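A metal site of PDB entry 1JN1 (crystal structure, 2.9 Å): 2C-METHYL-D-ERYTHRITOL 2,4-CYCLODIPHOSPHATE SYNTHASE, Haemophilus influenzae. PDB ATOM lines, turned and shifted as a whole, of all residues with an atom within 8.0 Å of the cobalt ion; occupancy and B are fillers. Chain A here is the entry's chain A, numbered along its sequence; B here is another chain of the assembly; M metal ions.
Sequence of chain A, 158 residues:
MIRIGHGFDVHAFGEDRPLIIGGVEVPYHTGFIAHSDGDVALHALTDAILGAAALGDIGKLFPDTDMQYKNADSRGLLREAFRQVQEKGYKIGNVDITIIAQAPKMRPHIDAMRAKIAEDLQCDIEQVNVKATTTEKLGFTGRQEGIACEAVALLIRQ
ND1 of His 43 lies close to O of Asp 39 (3.5 Å). A ring nitrogen (NE2) of His 43 sits at hydrogen-bond distance from the backbone carbonyl oxygen of Ala 34 (3.5 Å). The side-chain carboxylate (OE2) of Glu 136 of chain B is in hydrogen-bond range of a ring nitrogen (ND1) of His 11 (2.5 Å).
The nearest printed residue that does not touch the cobalt ion is Val 40 (4.8 Å).
The cobalt ion is bound by the side-chain carboxylate (OD1) of Asp 9 (2.0 Å), a ring nitrogen (ND1) of His 43 (2.1 Å), a ring nitrogen (ND1) of His 35 (2.2 Å) and a ring nitrogen (NE2) of His 11 (2.2 Å). The cobalt ion has four donor atoms within binding distance.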
ATOM      1  N   PHE A   8      17.952  10.611  16.974  1.00  0.00           N
ATOM      2  CA  PHE A   8      17.468   9.852  18.095  1.00  0.00           C
ATOM      3  C   PHE A   8      18.253   8.557  18.282  1.00  0.00           C
ATOM      4  O   PHE A   8      18.629   7.945  17.299  1.00  0.00           O
ATOM      5  CB  PHE A   8      15.990   9.592  17.807  1.00  0.00           C
ATOM      6  CG  PHE A   8      15.389   8.548  18.650  1.00  0.00           C
ATOM      7  CD1 PHE A   8      14.939   8.838  19.920  1.00  0.00           C
ATOM      8  CD2 PHE A   8      15.218   7.281  18.151  1.00  0.00           C
ATOM      9  CE1 PHE A   8      14.313   7.881  20.682  1.00  0.00           C
ATOM     10  CE2 PHE A   8      14.596   6.336  18.905  1.00  0.00           C
ATOM     11  CZ  PHE A   8      14.138   6.625  20.171  1.00  0.00           C
ATOM     12  N   ASP A   9      18.517   8.134  19.528  1.00  0.00           N
ATOM     13  CA  ASP A   9      19.277   6.908  19.794  1.00  0.00           C
ATOM     14  C   ASP A   9      18.883   6.194  21.056  1.00  0.00           C
ATOM     15  O   ASP A   9      18.633   6.812  22.101  1.00  0.00           O
ATOM     16  CB  ASP A   9      20.751   7.210  19.888  1.00  0.00           C
ATOM     17  CG  ASP A   9      21.614   6.077  19.413  1.00  0.00           C
ATOM     18  OD1 ASP A   9      22.830   6.171  19.685  1.00  0.00           O
ATOM     19  OD2 ASP A   9      21.137   5.108  18.765  1.00  0.00           O
ATOM     20  N   VAL A  10      18.818   4.876  20.936  1.00  0.00           N
ATOM     21  CA  VAL A  10      18.468   4.030  22.050  1.00  0.00           C
ATOM     22  C   VAL A  10      19.596   3.050  22.266  1.00  0.00           C
ATOM     23  O   VAL A  10      20.146   2.523  21.316  1.00  0.00           O
ATOM     24  CB  VAL A  10      17.203   3.234  21.771  1.00  0.00           C
ATOM     25  CG1 VAL A  10      17.140   2.081  22.730  1.00  0.00           C
ATOM     26  CG2 VAL A  10      15.967   4.101  21.929  1.00  0.00           C
ATOM     27  N   HIS A  11      20.010   2.805  23.500  1.00  0.00           N
ATOM     28  CA  HIS A  11      21.055   1.808  23.700  1.00  0.00           C
ATOM     29  C   HIS A  11      20.809   0.982  24.912  1.00  0.00           C
ATOM     30  O   HIS A  11      20.360   1.492  25.929  1.00  0.00           O
ATOM     31  CB  HIS A  11      22.438   2.436  23.868  1.00  0.00           C
ATOM     32  CG  HIS A  11      23.198   2.583  22.592  1.00  0.00           C
ATOM     33  ND1 HIS A  11      23.624   1.504  21.851  1.00  0.00           N
ATOM     34  CD2 HIS A  11      23.611   3.679  21.930  1.00  0.00           C
ATOM     35  CE1 HIS A  11      24.262   1.929  20.786  1.00  0.00           C
ATOM     36  NE2 HIS A  11      24.270   3.253  20.804  1.00  0.00           N
ATOM     37  N   HIS A  29      24.258  -4.832  12.544  1.00  0.00           N
ATOM     38  CA  HIS A  29      23.475  -3.889  11.797  1.00  0.00           C
ATOM     39  C   HIS A  29      24.555  -2.985  11.195  1.00  0.00           C
ATOM     40  O   HIS A  29      25.748  -3.301  11.315  1.00  0.00           O
ATOM     41  CB  HIS A  29      22.450  -3.152  12.696  1.00  0.00           C
ATOM     42  CG  HIS A  29      23.045  -2.188  13.679  1.00  0.00           C
ATOM     43  ND1 HIS A  29      22.842  -2.288  15.049  1.00  0.00           N
ATOM     44  CD2 HIS A  29      23.787  -1.062  13.503  1.00  0.00           C
ATOM     45  CE1 HIS A  29      23.421  -1.275  15.658  1.00  0.00           C
ATOM     46  NE2 HIS A  29      24.003  -0.509  14.746  1.00  0.00           N
ATOM     47  N   GLY A  31      25.622   0.897  11.274  1.00  0.00           N
ATOM     48  CA  GLY A  31      26.601   1.708  11.986  1.00  0.00           C
ATOM     49  C   GLY A  31      26.891   1.035  13.322  1.00  0.00           C
ATOM     50  O   GLY A  31      27.090   1.703  14.330  1.00  0.00           O
ATOM     51  N   PHE A  32      26.904  -0.289  13.327  1.00  0.00           N
ATOM     52  CA  PHE A  32      27.115  -1.010  14.563  1.00  0.00           C
ATOM     53  C   PHE A  32      28.369  -0.736  15.355  1.00  0.00           C
ATOM     54  O   PHE A  32      28.276  -0.544  16.557  1.00  0.00           O
ATOM     55  CB  PHE A  32      27.054  -2.502  14.370  1.00  0.00           C
ATOM     56  CG  PHE A  32      27.234  -3.250  15.642  1.00  0.00           C
ATOM     57  CD1 PHE A  32      26.130  -3.600  16.428  1.00  0.00           C
ATOM     58  CD2 PHE A  32      28.519  -3.514  16.115  1.00  0.00           C
ATOM     59  CE1 PHE A  32      26.321  -4.213  17.671  1.00  0.00           C
ATOM     60  CE2 PHE A  32      28.703  -4.124  17.331  1.00  0.00           C
ATOM     61  CZ  PHE A  32      27.607  -4.465  18.124  1.00  0.00           C
ATOM     62  N   ALA A  34      30.528   1.928  15.110  1.00  0.00           N
ATOM     63  CA  ALA A  34      30.540   3.324  15.574  1.00  0.00           C
ATOM     64  C   ALA A  34      29.659   3.571  16.834  1.00  0.00           C
ATOM     65  O   ALA A  34      30.025   4.373  17.704  1.00  0.00           O
ATOM     66  CB  ALA A  34      30.096   4.254  14.426  1.00  0.00           C
ATOM     67  N   HIS A  35      28.526   2.880  16.917  1.00  0.00           N
ATOM     68  CA  HIS A  35      27.585   2.967  18.011  1.00  0.00           C
ATOM     69  C   HIS A  35      28.048   2.162  19.237  1.00  0.00           C
ATOM     70  O   HIS A  35      27.725   2.513  20.347  1.00  0.00           O
ATOM     71  CB  HIS A  35      26.212   2.397  17.603  1.00  0.00           C
ATOM     72  CG  HIS A  35      25.366   3.312  16.769  1.00  0.00           C
ATOM     73  ND1 HIS A  35      24.594   4.326  17.312  1.00  0.00           N
ATOM     74  CD2 HIS A  35      25.193   3.411  15.427  1.00  0.00           C
ATOM     75  CE1 HIS A  35      24.005   4.998  16.351  1.00  0.00           C
ATOM     76  NE2 HIS A  35      24.352   4.473  15.192  1.00  0.00           N
ATOM     77  N   SER A  36      28.769   1.066  19.025  1.00  0.00           N
ATOM     78  CA  SER A  36      29.233   0.164  20.119  1.00  0.00           C
ATOM     79  C   SER A  36      29.532   0.805  21.472  1.00  0.00           C
ATOM     80  O   SER A  36      29.339   0.176  22.502  1.00  0.00           O
ATOM     81  CB  SER A  36      30.443  -0.666  19.684  1.00  0.00           C
ATOM     82  OG  SER A  36      31.496   0.183  19.291  1.00  0.00           O
ATOM     83  N   ASP A  37      30.037   2.025  21.419  1.00  0.00           N
ATOM     84  CA  ASP A  37      30.370   2.897  22.539  1.00  0.00           C
ATOM     85  C   ASP A  37      29.050   3.023  23.387  1.00  0.00           C
ATOM     86  O   ASP A  37      29.027   2.886  24.610  1.00  0.00           O
ATOM     87  CB  ASP A  37      30.793   4.173  21.808  1.00  0.00           C
ATOM     88  CG  ASP A  37      31.229   5.262  22.698  1.00  0.00           C
ATOM     89  OD1 ASP A  37      30.414   5.734  23.451  1.00  0.00           O
ATOM     90  OD2 ASP A  37      32.380   5.684  22.603  1.00  0.00           O
ATOM     91  N   GLY A  38      27.941   3.248  22.693  1.00  0.00           N
ATOM     92  CA  GLY A  38      26.649   3.360  23.333  1.00  0.00           C
ATOM     93  C   GLY A  38      26.388   4.707  23.993  1.00  0.00           C
ATOM     94  O   GLY A  38      25.589   4.837  24.919  1.00  0.00           O
ATOM     95  N   ASP A  39      27.009   5.737  23.474  1.00  0.00           N
ATOM     96  CA  ASP A  39      26.866   7.047  24.032  1.00  0.00           C
ATOM     97  C   ASP A  39      25.749   7.697  23.243  1.00  0.00           C
ATOM     98  O   ASP A  39      26.027   8.415  22.299  1.00  0.00           O
ATOM     99  CB  ASP A  39      28.229   7.646  23.798  1.00  0.00           C
ATOM    100  CG  ASP A  39      28.495   8.916  24.550  1.00  0.00           C
ATOM    101  OD1 ASP A  39      29.662   9.087  24.901  1.00  0.00           O
ATOM    102  OD2 ASP A  39      27.579   9.711  24.740  1.00  0.00           O
ATOM    103  N   VAL A  40      24.502   7.399  23.594  1.00  0.00           N
ATOM    104  CA  VAL A  40      23.326   7.952  22.894  1.00  0.00           C
ATOM    105  C   VAL A  40      23.381   9.447  22.781  1.00  0.00           C
ATOM    106  O   VAL A  40      22.772  10.027  21.899  1.00  0.00           O
ATOM    107  CB  VAL A  40      22.001   7.634  23.641  1.00  0.00           C
ATOM    108  CG1 VAL A  40      21.618   6.165  23.499  1.00  0.00           C
ATOM    109  CG2 VAL A  40      22.152   8.020  25.145  1.00  0.00           C
ATOM    110  N   ALA A  41      24.134  10.106  23.652  1.00  0.00           N
ATOM    111  CA  ALA A  41      24.143  11.558  23.599  1.00  0.00           C
ATOM    112  C   ALA A  41      24.930  12.076  22.472  1.00  0.00           C
ATOM    113  O   ALA A  41      24.474  12.940  21.726  1.00  0.00           O
ATOM    114  CB  ALA A  41      24.679  12.129  24.889  1.00  0.00           C
ATOM    115  N   LEU A  42      26.124  11.534  22.345  1.00  0.00           N
ATOM    116  CA  LEU A  42      26.997  11.992  21.292  1.00  0.00           C
ATOM    117  C   LEU A  42      26.526  11.495  19.946  1.00  0.00           C
ATOM    118  O   LEU A  42      26.546  12.274  18.946  1.00  0.00           O
ATOM    119  CB  LEU A  42      28.439  11.569  21.607  1.00  0.00           C
ATOM    120  CG  LEU A  42      29.041  12.120  22.944  1.00  0.00           C
ATOM    121  CD1 LEU A  42      30.389  11.540  23.132  1.00  0.00           C
ATOM    122  CD2 LEU A  42      29.143  13.647  22.945  1.00  0.00           C
ATOM    123  N   HIS A  43      26.013  10.245  19.895  1.00  0.00           N
ATOM    124  CA  HIS A  43      25.562   9.681  18.619  1.00  0.00           C
ATOM    125  C   HIS A  43      24.371  10.403  18.032  1.00  0.00           C
ATOM    126  O   HIS A  43      24.306  10.610  16.817  1.00  0.00           O
ATOM    127  CB  HIS A  43      25.222   8.171  18.705  1.00  0.00           C
ATOM    128  CG  HIS A  43      26.363   7.306  19.169  1.00  0.00           C
ATOM    129  ND1 HIS A  43      26.162   6.069  19.755  1.00  0.00           N
ATOM    130  CD2 HIS A  43      27.698   7.517  19.227  1.00  0.00           C
ATOM    131  CE1 HIS A  43      27.312   5.576  20.159  1.00  0.00           C
ATOM    132  NE2 HIS A  43      28.262   6.444  19.861  1.00  0.00           N
ATOM    133  N   ALA A  44      23.409  10.724  18.908  1.00  0.00           N
ATOM    134  CA  ALA A  44      22.175  11.379  18.519  1.00  0.00           C
ATOM    135  C   ALA A  44      22.469  12.758  18.022  1.00  0.00           C
ATOM    136  O   ALA A  44      21.954  13.162  16.990  1.00  0.00           O
ATOM    137  CB  ALA A  44      21.255  11.441  19.679  1.00  0.00           C
ATOM    138  N   ASP A  47      23.952  12.506  14.694  1.00  0.00           N
ATOM    139  CA  ASP A  47      22.904  12.238  13.766  1.00  0.00           C
ATOM    140  C   ASP A  47      22.190  13.533  13.457  1.00  0.00           C
ATOM    141  O   ASP A  47      21.781  13.736  12.335  1.00  0.00           O
ATOM    142  CB  ASP A  47      21.919  11.257  14.410  1.00  0.00           C
ATOM    143  CG  ASP A  47      22.040   9.832  13.878  1.00  0.00           C
ATOM    144  OD1 ASP A  47      23.065   9.479  13.254  1.00  0.00           O
ATOM    145  OD2 ASP A  47      21.058   9.059  14.104  1.00  0.00           O
ATOM    146  N   ILE A  58      24.967   8.609  10.879  1.00  0.00           N
ATOM    147  CA  ILE A  58      26.095   7.812  11.359  1.00  0.00           C
ATOM    148  C   ILE A  58      26.390   6.473  10.662  1.00  0.00           C
ATOM    149  O   ILE A  58      27.541   6.061  10.601  1.00  0.00           O
ATOM    150  CB  ILE A  58      25.919   7.529  12.854  1.00  0.00           C
ATOM    151  CG1 ILE A  58      26.271   8.773  13.639  1.00  0.00           C
ATOM    152  CG2 ILE A  58      26.777   6.346  13.288  1.00  0.00           C
ATOM    153  CD1 ILE A  58      26.088   8.559  15.142  1.00  0.00           C
ATOM    154  N   SER A  74      33.390   7.828  20.129  1.00  0.00           N
ATOM    155  CA  SER A  74      32.304   8.619  19.556  1.00  0.00           C
ATOM    156  C   SER A  74      32.436  10.121  19.628  1.00  0.00           C
ATOM    157  O   SER A  74      31.646  10.832  19.049  1.00  0.00           O
ATOM    158  CB  SER A  74      30.943   8.158  20.094  1.00  0.00           C
ATOM    159  OG  SER A  74      30.826   8.442  21.451  1.00  0.00           O
ATOM    160  N   THR B 133      17.552   4.165  12.137  1.00  0.00           N
ATOM    161  CA  THR B 133      18.218   3.526  13.322  1.00  0.00           C
ATOM    162  C   THR B 133      17.369   2.462  13.936  1.00  0.00           C
ATOM    163  O   THR B 133      16.174   2.367  13.688  1.00  0.00           O
ATOM    164  CB  THR B 133      18.382   4.370  14.537  1.00  0.00           C
ATOM    165  OG1 THR B 133      17.149   5.047  14.781  1.00  0.00           O
ATOM    166  CG2 THR B 133      19.566   5.292  14.430  1.00  0.00           C
ATOM    167  N   THR B 134      17.993   1.721  14.823  1.00  0.00           N
ATOM    168  CA  THR B 134      17.333   0.635  15.531  1.00  0.00           C
ATOM    169  C   THR B 134      17.364   1.033  17.004  1.00  0.00           C
ATOM    170  O   THR B 134      18.125   1.936  17.407  1.00  0.00           O
ATOM    171  CB  THR B 134      18.099  -0.673  15.355  1.00  0.00           C
ATOM    172  OG1 THR B 134      19.080  -0.776  16.381  1.00  0.00           O
ATOM    173  CG2 THR B 134      18.837  -0.711  13.990  1.00  0.00           C
ATOM    174  N   GLU B 136      18.200  -0.973  19.479  1.00  0.00           N
ATOM    175  CA  GLU B 136      18.938  -2.067  20.092  1.00  0.00           C
ATOM    176  C   GLU B 136      18.033  -3.022  20.856  1.00  0.00           C
ATOM    177  O   GLU B 136      18.262  -3.320  22.034  1.00  0.00           O
ATOM    178  CB  GLU B 136      20.020  -1.480  21.000  1.00  0.00           C
ATOM    179  CG  GLU B 136      21.001  -2.469  21.527  1.00  0.00           C
ATOM    180  CD  GLU B 136      22.296  -1.821  21.984  1.00  0.00           C
ATOM    181  OE1 GLU B 136      23.099  -2.446  22.714  1.00  0.00           O
ATOM    182  OE2 GLU B 136      22.504  -0.667  21.611  1.00  0.00           O
HETATM  183 CO    CO M   1      24.387   4.918  19.379  1.00  0.00          CO
